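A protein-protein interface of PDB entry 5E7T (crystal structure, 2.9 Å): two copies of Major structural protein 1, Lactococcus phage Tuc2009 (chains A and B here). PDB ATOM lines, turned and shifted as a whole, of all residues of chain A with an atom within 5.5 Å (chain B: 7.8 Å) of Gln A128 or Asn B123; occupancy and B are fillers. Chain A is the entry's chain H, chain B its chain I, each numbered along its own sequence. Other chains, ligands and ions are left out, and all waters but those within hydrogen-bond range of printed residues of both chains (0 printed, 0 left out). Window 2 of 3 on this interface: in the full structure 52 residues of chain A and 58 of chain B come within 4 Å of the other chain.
O of Gly A94 lies within hydrogen-bond range of N of Ile A130 (3.0 Å). A ring nitrogen (NE2) of His B125 sits at hydrogen-bond distance from the backbone carbonyl oxygen (O) of Gly B94, at 3.3 Å. The backbone NH (N) of Ile B130 is in hydrogen-bond range of the backbone carbonyl oxygen (O) of Gly B94, 3.0 Å away. The side-chain hydroxyl (OH) of Tyr B121 is in hydrogen-bond range of the side-chain carboxylate (OE2) of Glu B101 (3.1 Å). OG1 of Thr B122 sits close to NE2 of His B125. ND1 of His B125 is in hydrogen-bond range of O of Asn B123, at 2.9 Å.
NZ of Lys A162 lies within salt-bridge range of OE2 of Glu B101 (2.9 Å). NZ of Lys A162 sits at hydrogen-bond distance from OH of Tyr B121.
Gln A128 touches two residues of chain B. Asn B123 touches three residues of chain A. Printed residues of chain A within 4 Å of Tyr B121: Ala A129 and Lys A162. Of the printed residues of chain A, His B125 touches Ile A130 (3.3 Å). Asp B126 touches none of the printed residues of chain A. Gly B94 touches none of the printed residues of chain A. The nearest residue of chain A that does not touch Asn B123 is Asn A127 (4.6 Å).
Ile A130 touches His B125, but with the chains exchanged His A125 does not touch Ile B130 (7.3 Å). Ile A130 touches its own counterpart, Ile B130. Of the 9 pairs that touch across the chains among the printed residues, 1 has its exchanged pair printed and touching as well.
Among the printed residues, pairs that only touch across the chains: Gln A128 with Asn B123, Gln A128 with Gly B124, Ala A129 with Tyr B121, Ala A129 with Asn B123, Ile A130 with Asn B123, Ile A130 with His B125 and Ile A130 with Ile B130.
Hydrophobic or aromatic side chains of chain A within 4 Å of the printed part of chain B: Ala A129 and Ile A130. Of the 17 printed residues of chain B, 6 touch a printed residue of chain A. Hydrophobic or aromatic side chains of chain B that line the printed part of chain A: Tyr B121, His B125 and Ile B130. Among the printed residues, Asp or Glu carboxylates within 4 Å of a Lys or Arg side-chain nitrogen of the other chain: Lys A162 with Glu B101 (2.9 Å).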
ATOM      1  N   GLY A  94     -19.773 -22.331  -1.404  1.00  0.00           N
ATOM      2  CA  GLY A  94     -19.623 -21.314  -0.366  1.00  0.00           C
ATOM      3  C   GLY A  94     -18.213 -20.872  -0.032  1.00  0.00           C
ATOM      4  O   GLY A  94     -17.283 -21.079  -0.815  1.00  0.00           O
ATOM      5  N   TRP A  95     -18.070 -20.236   1.148  1.00  0.00           N
ATOM      6  CA  TRP A  95     -16.819 -19.717   1.713  1.00  0.00           C
ATOM      7  C   TRP A  95     -16.872 -19.716   3.251  1.00  0.00           C
ATOM      8  O   TRP A  95     -17.943 -19.510   3.828  1.00  0.00           O
ATOM      9  CB  TRP A  95     -16.505 -18.295   1.169  1.00  0.00           C
ATOM     10  CG  TRP A  95     -17.370 -17.180   1.709  1.00  0.00           C
ATOM     11  CD1 TRP A  95     -17.111 -16.400   2.798  1.00  0.00           C
ATOM     12  CD2 TRP A  95     -18.611 -16.704   1.163  1.00  0.00           C
ATOM     13  NE1 TRP A  95     -18.127 -15.490   2.986  1.00  0.00           N
ATOM     14  CE2 TRP A  95     -19.068 -15.663   2.004  1.00  0.00           C
ATOM     15  CE3 TRP A  95     -19.396 -17.071   0.055  1.00  0.00           C
ATOM     16  CZ2 TRP A  95     -20.260 -14.969   1.759  1.00  0.00           C
ATOM     17  CZ3 TRP A  95     -20.581 -16.386  -0.181  1.00  0.00           C
ATOM     18  CH2 TRP A  95     -21.004 -15.354   0.666  1.00  0.00           C
ATOM     19  N   HIS A 125     -10.713 -17.368  -0.349  1.00  0.00           N
ATOM     20  CA  HIS A 125     -11.646 -16.714  -1.286  1.00  0.00           C
ATOM     21  C   HIS A 125     -12.913 -16.109  -0.599  1.00  0.00           C
ATOM     22  O   HIS A 125     -14.045 -16.481  -0.926  1.00  0.00           O
ATOM     23  CB  HIS A 125     -12.011 -17.668  -2.450  1.00  0.00           C
ATOM     24  CG  HIS A 125     -12.692 -18.936  -2.022  1.00  0.00           C
ATOM     25  ND1 HIS A 125     -11.980 -20.096  -1.786  1.00  0.00           N
ATOM     26  CD2 HIS A 125     -14.000 -19.173  -1.771  1.00  0.00           C
ATOM     27  CE1 HIS A 125     -12.876 -20.993  -1.408  1.00  0.00           C
ATOM     28  NE2 HIS A 125     -14.102 -20.483  -1.381  1.00  0.00           N
ATOM     29  N   ASP A 126     -12.709 -15.169   0.350  1.00  0.00           N
ATOM     30  CA  ASP A 126     -13.794 -14.522   1.109  1.00  0.00           C
ATOM     31  C   ASP A 126     -14.831 -13.806   0.219  1.00  0.00           C
ATOM     32  O   ASP A 126     -14.459 -13.099  -0.722  1.00  0.00           O
ATOM     33  CB  ASP A 126     -13.239 -13.576   2.195  1.00  0.00           C
ATOM     34  CG  ASP A 126     -14.293 -12.971   3.112  1.00  0.00           C
ATOM     35  OD1 ASP A 126     -15.120 -13.739   3.659  1.00  0.00           O
ATOM     36  OD2 ASP A 126     -14.282 -11.731   3.292  1.00  0.00           O
ATOM     37  N   ASN A 127     -16.134 -14.019   0.537  1.00  0.00           N
ATOM     38  CA  ASN A 127     -17.334 -13.497  -0.143  1.00  0.00           C
ATOM     39  C   ASN A 127     -17.341 -13.811  -1.666  1.00  0.00           C
ATOM     40  O   ASN A 127     -17.647 -12.961  -2.510  1.00  0.00           O
ATOM     41  CB  ASN A 127     -17.586 -12.017   0.172  1.00  0.00           C
ATOM     42  CG  ASN A 127     -18.358 -11.820   1.458  1.00  0.00           C
ATOM     43  OD1 ASN A 127     -17.803 -11.845   2.561  1.00  0.00           O
ATOM     44  ND2 ASN A 127     -19.663 -11.632   1.347  1.00  0.00           N
ATOM     45  N   GLN A 128     -17.017 -15.081  -1.971  1.00  0.00           N
ATOM     46  CA  GLN A 128     -16.964 -15.739  -3.280  1.00  0.00           C
ATOM     47  C   GLN A 128     -17.287 -17.213  -2.977  1.00  0.00           C
ATOM     48  O   GLN A 128     -16.643 -17.795  -2.102  1.00  0.00           O
ATOM     49  CB  GLN A 128     -15.547 -15.640  -3.896  1.00  0.00           C
ATOM     50  CG  GLN A 128     -15.090 -14.243  -4.315  1.00  0.00           C
ATOM     51  CD  GLN A 128     -13.664 -14.223  -4.824  1.00  0.00           C
ATOM     52  OE1 GLN A 128     -12.746 -14.819  -4.242  1.00  0.00           O
ATOM     53  NE2 GLN A 128     -13.438 -13.495  -5.908  1.00  0.00           N
ATOM     54  N   ALA A 129     -18.289 -17.806  -3.652  1.00  0.00           N
ATOM     55  CA  ALA A 129     -18.680 -19.202  -3.388  1.00  0.00           C
ATOM     56  C   ALA A 129     -18.073 -20.225  -4.366  1.00  0.00           C
ATOM     57  O   ALA A 129     -18.324 -20.161  -5.571  1.00  0.00           O
ATOM     58  CB  ALA A 129     -20.195 -19.329  -3.339  1.00  0.00           C
ATOM     59  N   ILE A 130     -17.260 -21.159  -3.830  1.00  0.00           N
ATOM     60  CA  ILE A 130     -16.569 -22.223  -4.583  1.00  0.00           C
ATOM     61  C   ILE A 130     -17.222 -23.590  -4.287  1.00  0.00           C
ATOM     62  O   ILE A 130     -17.743 -23.773  -3.181  1.00  0.00           O
ATOM     63  CB  ILE A 130     -15.030 -22.187  -4.265  1.00  0.00           C
ATOM     64  CG1 ILE A 130     -14.342 -20.937  -4.860  1.00  0.00           C
ATOM     65  CG2 ILE A 130     -14.273 -23.465  -4.642  1.00  0.00           C
ATOM     66  CD1 ILE A 130     -14.408 -20.770  -6.380  1.00  0.00           C
ATOM     67  N   LYS A 162     -24.500 -20.484  -1.312  1.00  0.00           N
ATOM     68  CA  LYS A 162     -24.986 -20.003  -2.621  1.00  0.00           C
ATOM     69  C   LYS A 162     -25.237 -21.202  -3.551  1.00  0.00           C
ATOM     70  O   LYS A 162     -24.372 -22.069  -3.682  1.00  0.00           O
ATOM     71  CB  LYS A 162     -24.010 -18.992  -3.259  1.00  0.00           C
ATOM     72  CG  LYS A 162     -24.691 -17.760  -3.850  1.00  0.00           C
ATOM     73  CD  LYS A 162     -24.452 -17.669  -5.352  1.00  0.00           C
ATOM     74  CE  LYS A 162     -25.081 -16.467  -5.998  1.00  0.00           C
ATOM     75  NZ  LYS A 162     -24.198 -15.284  -5.893  1.00  0.00           N
ATOM     76  N   GLY B  94     -13.749 -24.694 -14.401  1.00  0.00           N
ATOM     77  CA  GLY B  94     -13.638 -23.432 -15.132  1.00  0.00           C
ATOM     78  C   GLY B  94     -13.593 -22.163 -14.305  1.00  0.00           C
ATOM     79  O   GLY B  94     -13.311 -22.201 -13.104  1.00  0.00           O
ATOM     80  N   TRP B  95     -13.860 -21.023 -14.978  1.00  0.00           N
ATOM     81  CA  TRP B  95     -13.886 -19.667 -14.412  1.00  0.00           C
ATOM     82  C   TRP B  95     -14.860 -18.767 -15.201  1.00  0.00           C
ATOM     83  O   TRP B  95     -15.005 -18.940 -16.412  1.00  0.00           O
ATOM     84  CB  TRP B  95     -12.461 -19.045 -14.371  1.00  0.00           C
ATOM     85  CG  TRP B  95     -11.900 -18.626 -15.705  1.00  0.00           C
ATOM     86  CD1 TRP B  95     -12.004 -17.397 -16.287  1.00  0.00           C
ATOM     87  CD2 TRP B  95     -11.120 -19.430 -16.604  1.00  0.00           C
ATOM     88  NE1 TRP B  95     -11.372 -17.394 -17.508  1.00  0.00           N
ATOM     89  CE2 TRP B  95     -10.832 -18.634 -17.735  1.00  0.00           C
ATOM     90  CE3 TRP B  95     -10.654 -20.755 -16.577  1.00  0.00           C
ATOM     91  CZ2 TRP B  95     -10.077 -19.113 -18.816  1.00  0.00           C
ATOM     92  CZ3 TRP B  95      -9.911 -21.228 -17.649  1.00  0.00           C
ATOM     93  CH2 TRP B  95      -9.631 -20.415 -18.752  1.00  0.00           C
ATOM     94  N   GLY B  96     -15.493 -17.815 -14.513  1.00  0.00           N
ATOM     95  CA  GLY B  96     -16.400 -16.850 -15.131  1.00  0.00           C
ATOM     96  C   GLY B  96     -15.622 -15.825 -15.933  1.00  0.00           C
ATOM     97  O   GLY B  96     -14.460 -15.557 -15.611  1.00  0.00           O
ATOM     98  N   GLY B  99     -13.246 -13.135 -14.398  1.00  0.00           N
ATOM     99  CA  GLY B  99     -13.534 -13.431 -13.000  1.00  0.00           C
ATOM    100  C   GLY B  99     -15.027 -13.379 -12.727  1.00  0.00           C
ATOM    101  O   GLY B  99     -15.824 -13.083 -13.623  1.00  0.00           O
ATOM    102  N   GLY B 100     -15.407 -13.681 -11.495  1.00  0.00           N
ATOM    103  CA  GLY B 100     -16.804 -13.641 -11.084  1.00  0.00           C
ATOM    104  C   GLY B 100     -17.675 -14.829 -11.455  1.00  0.00           C
ATOM    105  O   GLY B 100     -17.189 -15.889 -11.866  1.00  0.00           O
ATOM    106  N   GLU B 101     -18.990 -14.617 -11.302  1.00  0.00           N
ATOM    107  CA  GLU B 101     -20.098 -15.554 -11.476  1.00  0.00           C
ATOM    108  C   GLU B 101     -20.150 -16.295 -12.811  1.00  0.00           C
ATOM    109  O   GLU B 101     -19.787 -15.748 -13.855  1.00  0.00           O
ATOM    110  CB  GLU B 101     -21.442 -14.846 -11.233  1.00  0.00           C
ATOM    111  CG  GLU B 101     -21.571 -14.216  -9.858  1.00  0.00           C
ATOM    112  CD  GLU B 101     -22.955 -13.732  -9.484  1.00  0.00           C
ATOM    113  OE1 GLU B 101     -23.509 -12.878 -10.214  1.00  0.00           O
ATOM    114  OE2 GLU B 101     -23.465 -14.172  -8.428  1.00  0.00           O
ATOM    115  N   TRP B 102     -20.624 -17.562 -12.736  1.00  0.00           N
ATOM    116  CA  TRP B 102     -20.886 -18.533 -13.801  1.00  0.00           C
ATOM    117  C   TRP B 102     -21.585 -19.752 -13.176  1.00  0.00           C
ATOM    118  O   TRP B 102     -21.042 -20.373 -12.256  1.00  0.00           O
ATOM    119  CB  TRP B 102     -19.612 -18.957 -14.572  1.00  0.00           C
ATOM    120  CG  TRP B 102     -19.875 -19.783 -15.809  1.00  0.00           C
ATOM    121  CD1 TRP B 102     -21.053 -19.900 -16.488  1.00  0.00           C
ATOM    122  CD2 TRP B 102     -18.919 -20.577 -16.527  1.00  0.00           C
ATOM    123  NE1 TRP B 102     -20.899 -20.738 -17.564  1.00  0.00           N
ATOM    124  CE2 TRP B 102     -19.600 -21.167 -17.615  1.00  0.00           C
ATOM    125  CE3 TRP B 102     -17.556 -20.864 -16.346  1.00  0.00           C
ATOM    126  CZ2 TRP B 102     -18.957 -22.007 -18.534  1.00  0.00           C
ATOM    127  CZ3 TRP B 102     -16.920 -21.696 -17.258  1.00  0.00           C
ATOM    128  CH2 TRP B 102     -17.614 -22.245 -18.346  1.00  0.00           C
ATOM    129  N   TYR B 121     -21.862 -23.691  -9.561  1.00  0.00           N
ATOM    130  CA  TYR B 121     -21.455 -22.285  -9.429  1.00  0.00           C
ATOM    131  C   TYR B 121     -19.943 -22.089  -9.186  1.00  0.00           C
ATOM    132  O   TYR B 121     -19.303 -22.908  -8.524  1.00  0.00           O
ATOM    133  CB  TYR B 121     -22.308 -21.611  -8.325  1.00  0.00           C
ATOM    134  CG  TYR B 121     -22.023 -20.145  -8.052  1.00  0.00           C
ATOM    135  CD1 TYR B 121     -22.553 -19.143  -8.864  1.00  0.00           C
ATOM    136  CD2 TYR B 121     -21.296 -19.756  -6.933  1.00  0.00           C
ATOM    137  CE1 TYR B 121     -22.326 -17.791  -8.592  1.00  0.00           C
ATOM    138  CE2 TYR B 121     -21.045 -18.410  -6.663  1.00  0.00           C
ATOM    139  CZ  TYR B 121     -21.565 -17.430  -7.490  1.00  0.00           C
ATOM    140  OH  TYR B 121     -21.319 -16.109  -7.196  1.00  0.00           O
ATOM    141  N   THR B 122     -19.384 -20.988  -9.738  1.00  0.00           N
ATOM    142  CA  THR B 122     -17.977 -20.575  -9.614  1.00  0.00           C
ATOM    143  C   THR B 122     -17.892 -19.033  -9.517  1.00  0.00           C
ATOM    144  O   THR B 122     -18.772 -18.344 -10.041  1.00  0.00           O
ATOM    145  CB  THR B 122     -17.108 -21.224 -10.721  1.00  0.00           C
ATOM    146  OG1 THR B 122     -15.773 -21.391 -10.249  1.00  0.00           O
ATOM    147  CG2 THR B 122     -17.128 -20.462 -12.044  1.00  0.00           C
ATOM    148  N   ASN B 123     -16.851 -18.504  -8.832  1.00  0.00           N
ATOM    149  CA  ASN B 123     -16.639 -17.060  -8.605  1.00  0.00           C
ATOM    150  C   ASN B 123     -15.135 -16.726  -8.482  1.00  0.00           C
ATOM    151  O   ASN B 123     -14.393 -17.480  -7.847  1.00  0.00           O
ATOM    152  CB  ASN B 123     -17.383 -16.635  -7.316  1.00  0.00           C
ATOM    153  CG  ASN B 123     -17.810 -15.183  -7.212  1.00  0.00           C
ATOM    154  OD1 ASN B 123     -17.185 -14.262  -7.755  1.00  0.00           O
ATOM    155  ND2 ASN B 123     -18.860 -14.945  -6.438  1.00  0.00           N
ATOM    156  N   GLY B 124     -14.718 -15.598  -9.070  1.00  0.00           N
ATOM    157  CA  GLY B 124     -13.337 -15.106  -9.051  1.00  0.00           C
ATOM    158  C   GLY B 124     -12.338 -15.961  -9.808  1.00  0.00           C
ATOM    159  O   GLY B 124     -12.691 -16.558 -10.830  1.00  0.00           O
ATOM    160  N   HIS B 125     -11.078 -16.032  -9.295  1.00  0.00           N
ATOM    161  CA  HIS B 125      -9.928 -16.798  -9.815  1.00  0.00           C
ATOM    162  C   HIS B 125      -9.831 -16.806 -11.369  1.00  0.00           C
ATOM    163  O   HIS B 125      -9.844 -17.871 -11.993  1.00  0.00           O
ATOM    164  CB  HIS B 125      -9.902 -18.226  -9.226  1.00  0.00           C
ATOM    165  CG  HIS B 125     -11.117 -19.052  -9.547  1.00  0.00           C
ATOM    166  ND1 HIS B 125     -12.199 -19.116  -8.689  1.00  0.00           N
ATOM    167  CD2 HIS B 125     -11.388 -19.801 -10.641  1.00  0.00           C
ATOM    168  CE1 HIS B 125     -13.082 -19.897  -9.287  1.00  0.00           C
ATOM    169  NE2 HIS B 125     -12.639 -20.330 -10.463  1.00  0.00           N
ATOM    170  N   ASP B 126      -9.724 -15.602 -11.983  1.00  0.00           N
ATOM    171  CA  ASP B 126      -9.653 -15.433 -13.445  1.00  0.00           C
ATOM    172  C   ASP B 126      -8.484 -16.197 -14.098  1.00  0.00           C
ATOM    173  O   ASP B 126      -7.361 -16.165 -13.586  1.00  0.00           O
ATOM    174  CB  ASP B 126      -9.639 -13.945 -13.837  1.00  0.00           C
ATOM    175  CG  ASP B 126      -9.693 -13.684 -15.335  1.00  0.00           C
ATOM    176  OD1 ASP B 126     -10.590 -14.252 -16.008  1.00  0.00           O
ATOM    177  OD2 ASP B 126      -8.845 -12.905 -15.834  1.00  0.00           O
ATOM    178  N   GLN B 128      -7.961 -19.504 -14.367  1.00  0.00           N
ATOM    179  CA  GLN B 128      -7.630 -20.611 -13.467  1.00  0.00           C
ATOM    180  C   GLN B 128      -8.944 -21.412 -13.370  1.00  0.00           C
ATOM    181  O   GLN B 128      -9.984 -20.820 -13.074  1.00  0.00           O
ATOM    182  CB  GLN B 128      -7.236 -20.088 -12.065  1.00  0.00           C
ATOM    183  CG  GLN B 128      -5.912 -19.321 -11.982  1.00  0.00           C
ATOM    184  CD  GLN B 128      -5.635 -18.754 -10.608  1.00  0.00           C
ATOM    185  OE1 GLN B 128      -6.515 -18.198  -9.939  1.00  0.00           O
ATOM    186  NE2 GLN B 128      -4.386 -18.848 -10.171  1.00  0.00           N
ATOM    187  N   ILE B 130     -11.441 -24.033 -11.613  1.00  0.00           N
ATOM    188  CA  ILE B 130     -11.821 -24.650 -10.330  1.00  0.00           C
ATOM    189  C   ILE B 130     -13.021 -25.600 -10.527  1.00  0.00           C
ATOM    190  O   ILE B 130     -13.840 -25.342 -11.419  1.00  0.00           O
ATOM    191  CB  ILE B 130     -12.080 -23.529  -9.255  1.00  0.00           C
ATOM    192  CG1 ILE B 130     -10.770 -22.803  -8.838  1.00  0.00           C
ATOM    193  CG2 ILE B 130     -12.874 -24.002  -8.018  1.00  0.00           C
ATOM    194  CD1 ILE B 130      -9.655 -23.654  -8.221  1.00  0.00           C
ATOM    195  N   SER B 131     -13.124 -26.682  -9.703  1.00  0.00           N
ATOM    196  CA  SER B 131     -14.239 -27.636  -9.773  1.00  0.00           C
ATOM    197  C   SER B 131     -15.594 -26.949  -9.607  1.00  0.00           C
ATOM    198  O   SER B 131     -15.742 -26.047  -8.779  1.00  0.00           O
ATOM    199  CB  SER B 131     -14.086 -28.754  -8.748  1.00  0.00           C
ATOM    200  OG  SER B 131     -15.137 -29.704  -8.824  1.00  0.00           O
ATOM    201  N   MET B 132     -16.549 -27.341 -10.462  1.00  0.00           N
ATOM    202  CA  MET B 132     -17.920 -26.829 -10.509  1.00  0.00           C
ATOM    203  C   MET B 132     -18.852 -27.922 -11.097  1.00  0.00           C
ATOM    204  O   MET B 132     -19.470 -27.698 -12.143  1.00  0.00           O
ATOM    205  CB  MET B 132     -17.996 -25.464 -11.268  1.00  0.00           C
ATOM    206  CG  MET B 132     -17.391 -25.479 -12.682  1.00  0.00           C
ATOM    207  SD  MET B 132     -17.239 -23.863 -13.479  1.00  0.00           S
ATOM    208  CE  MET B 132     -18.932 -23.427 -13.710  1.00  0.00           C
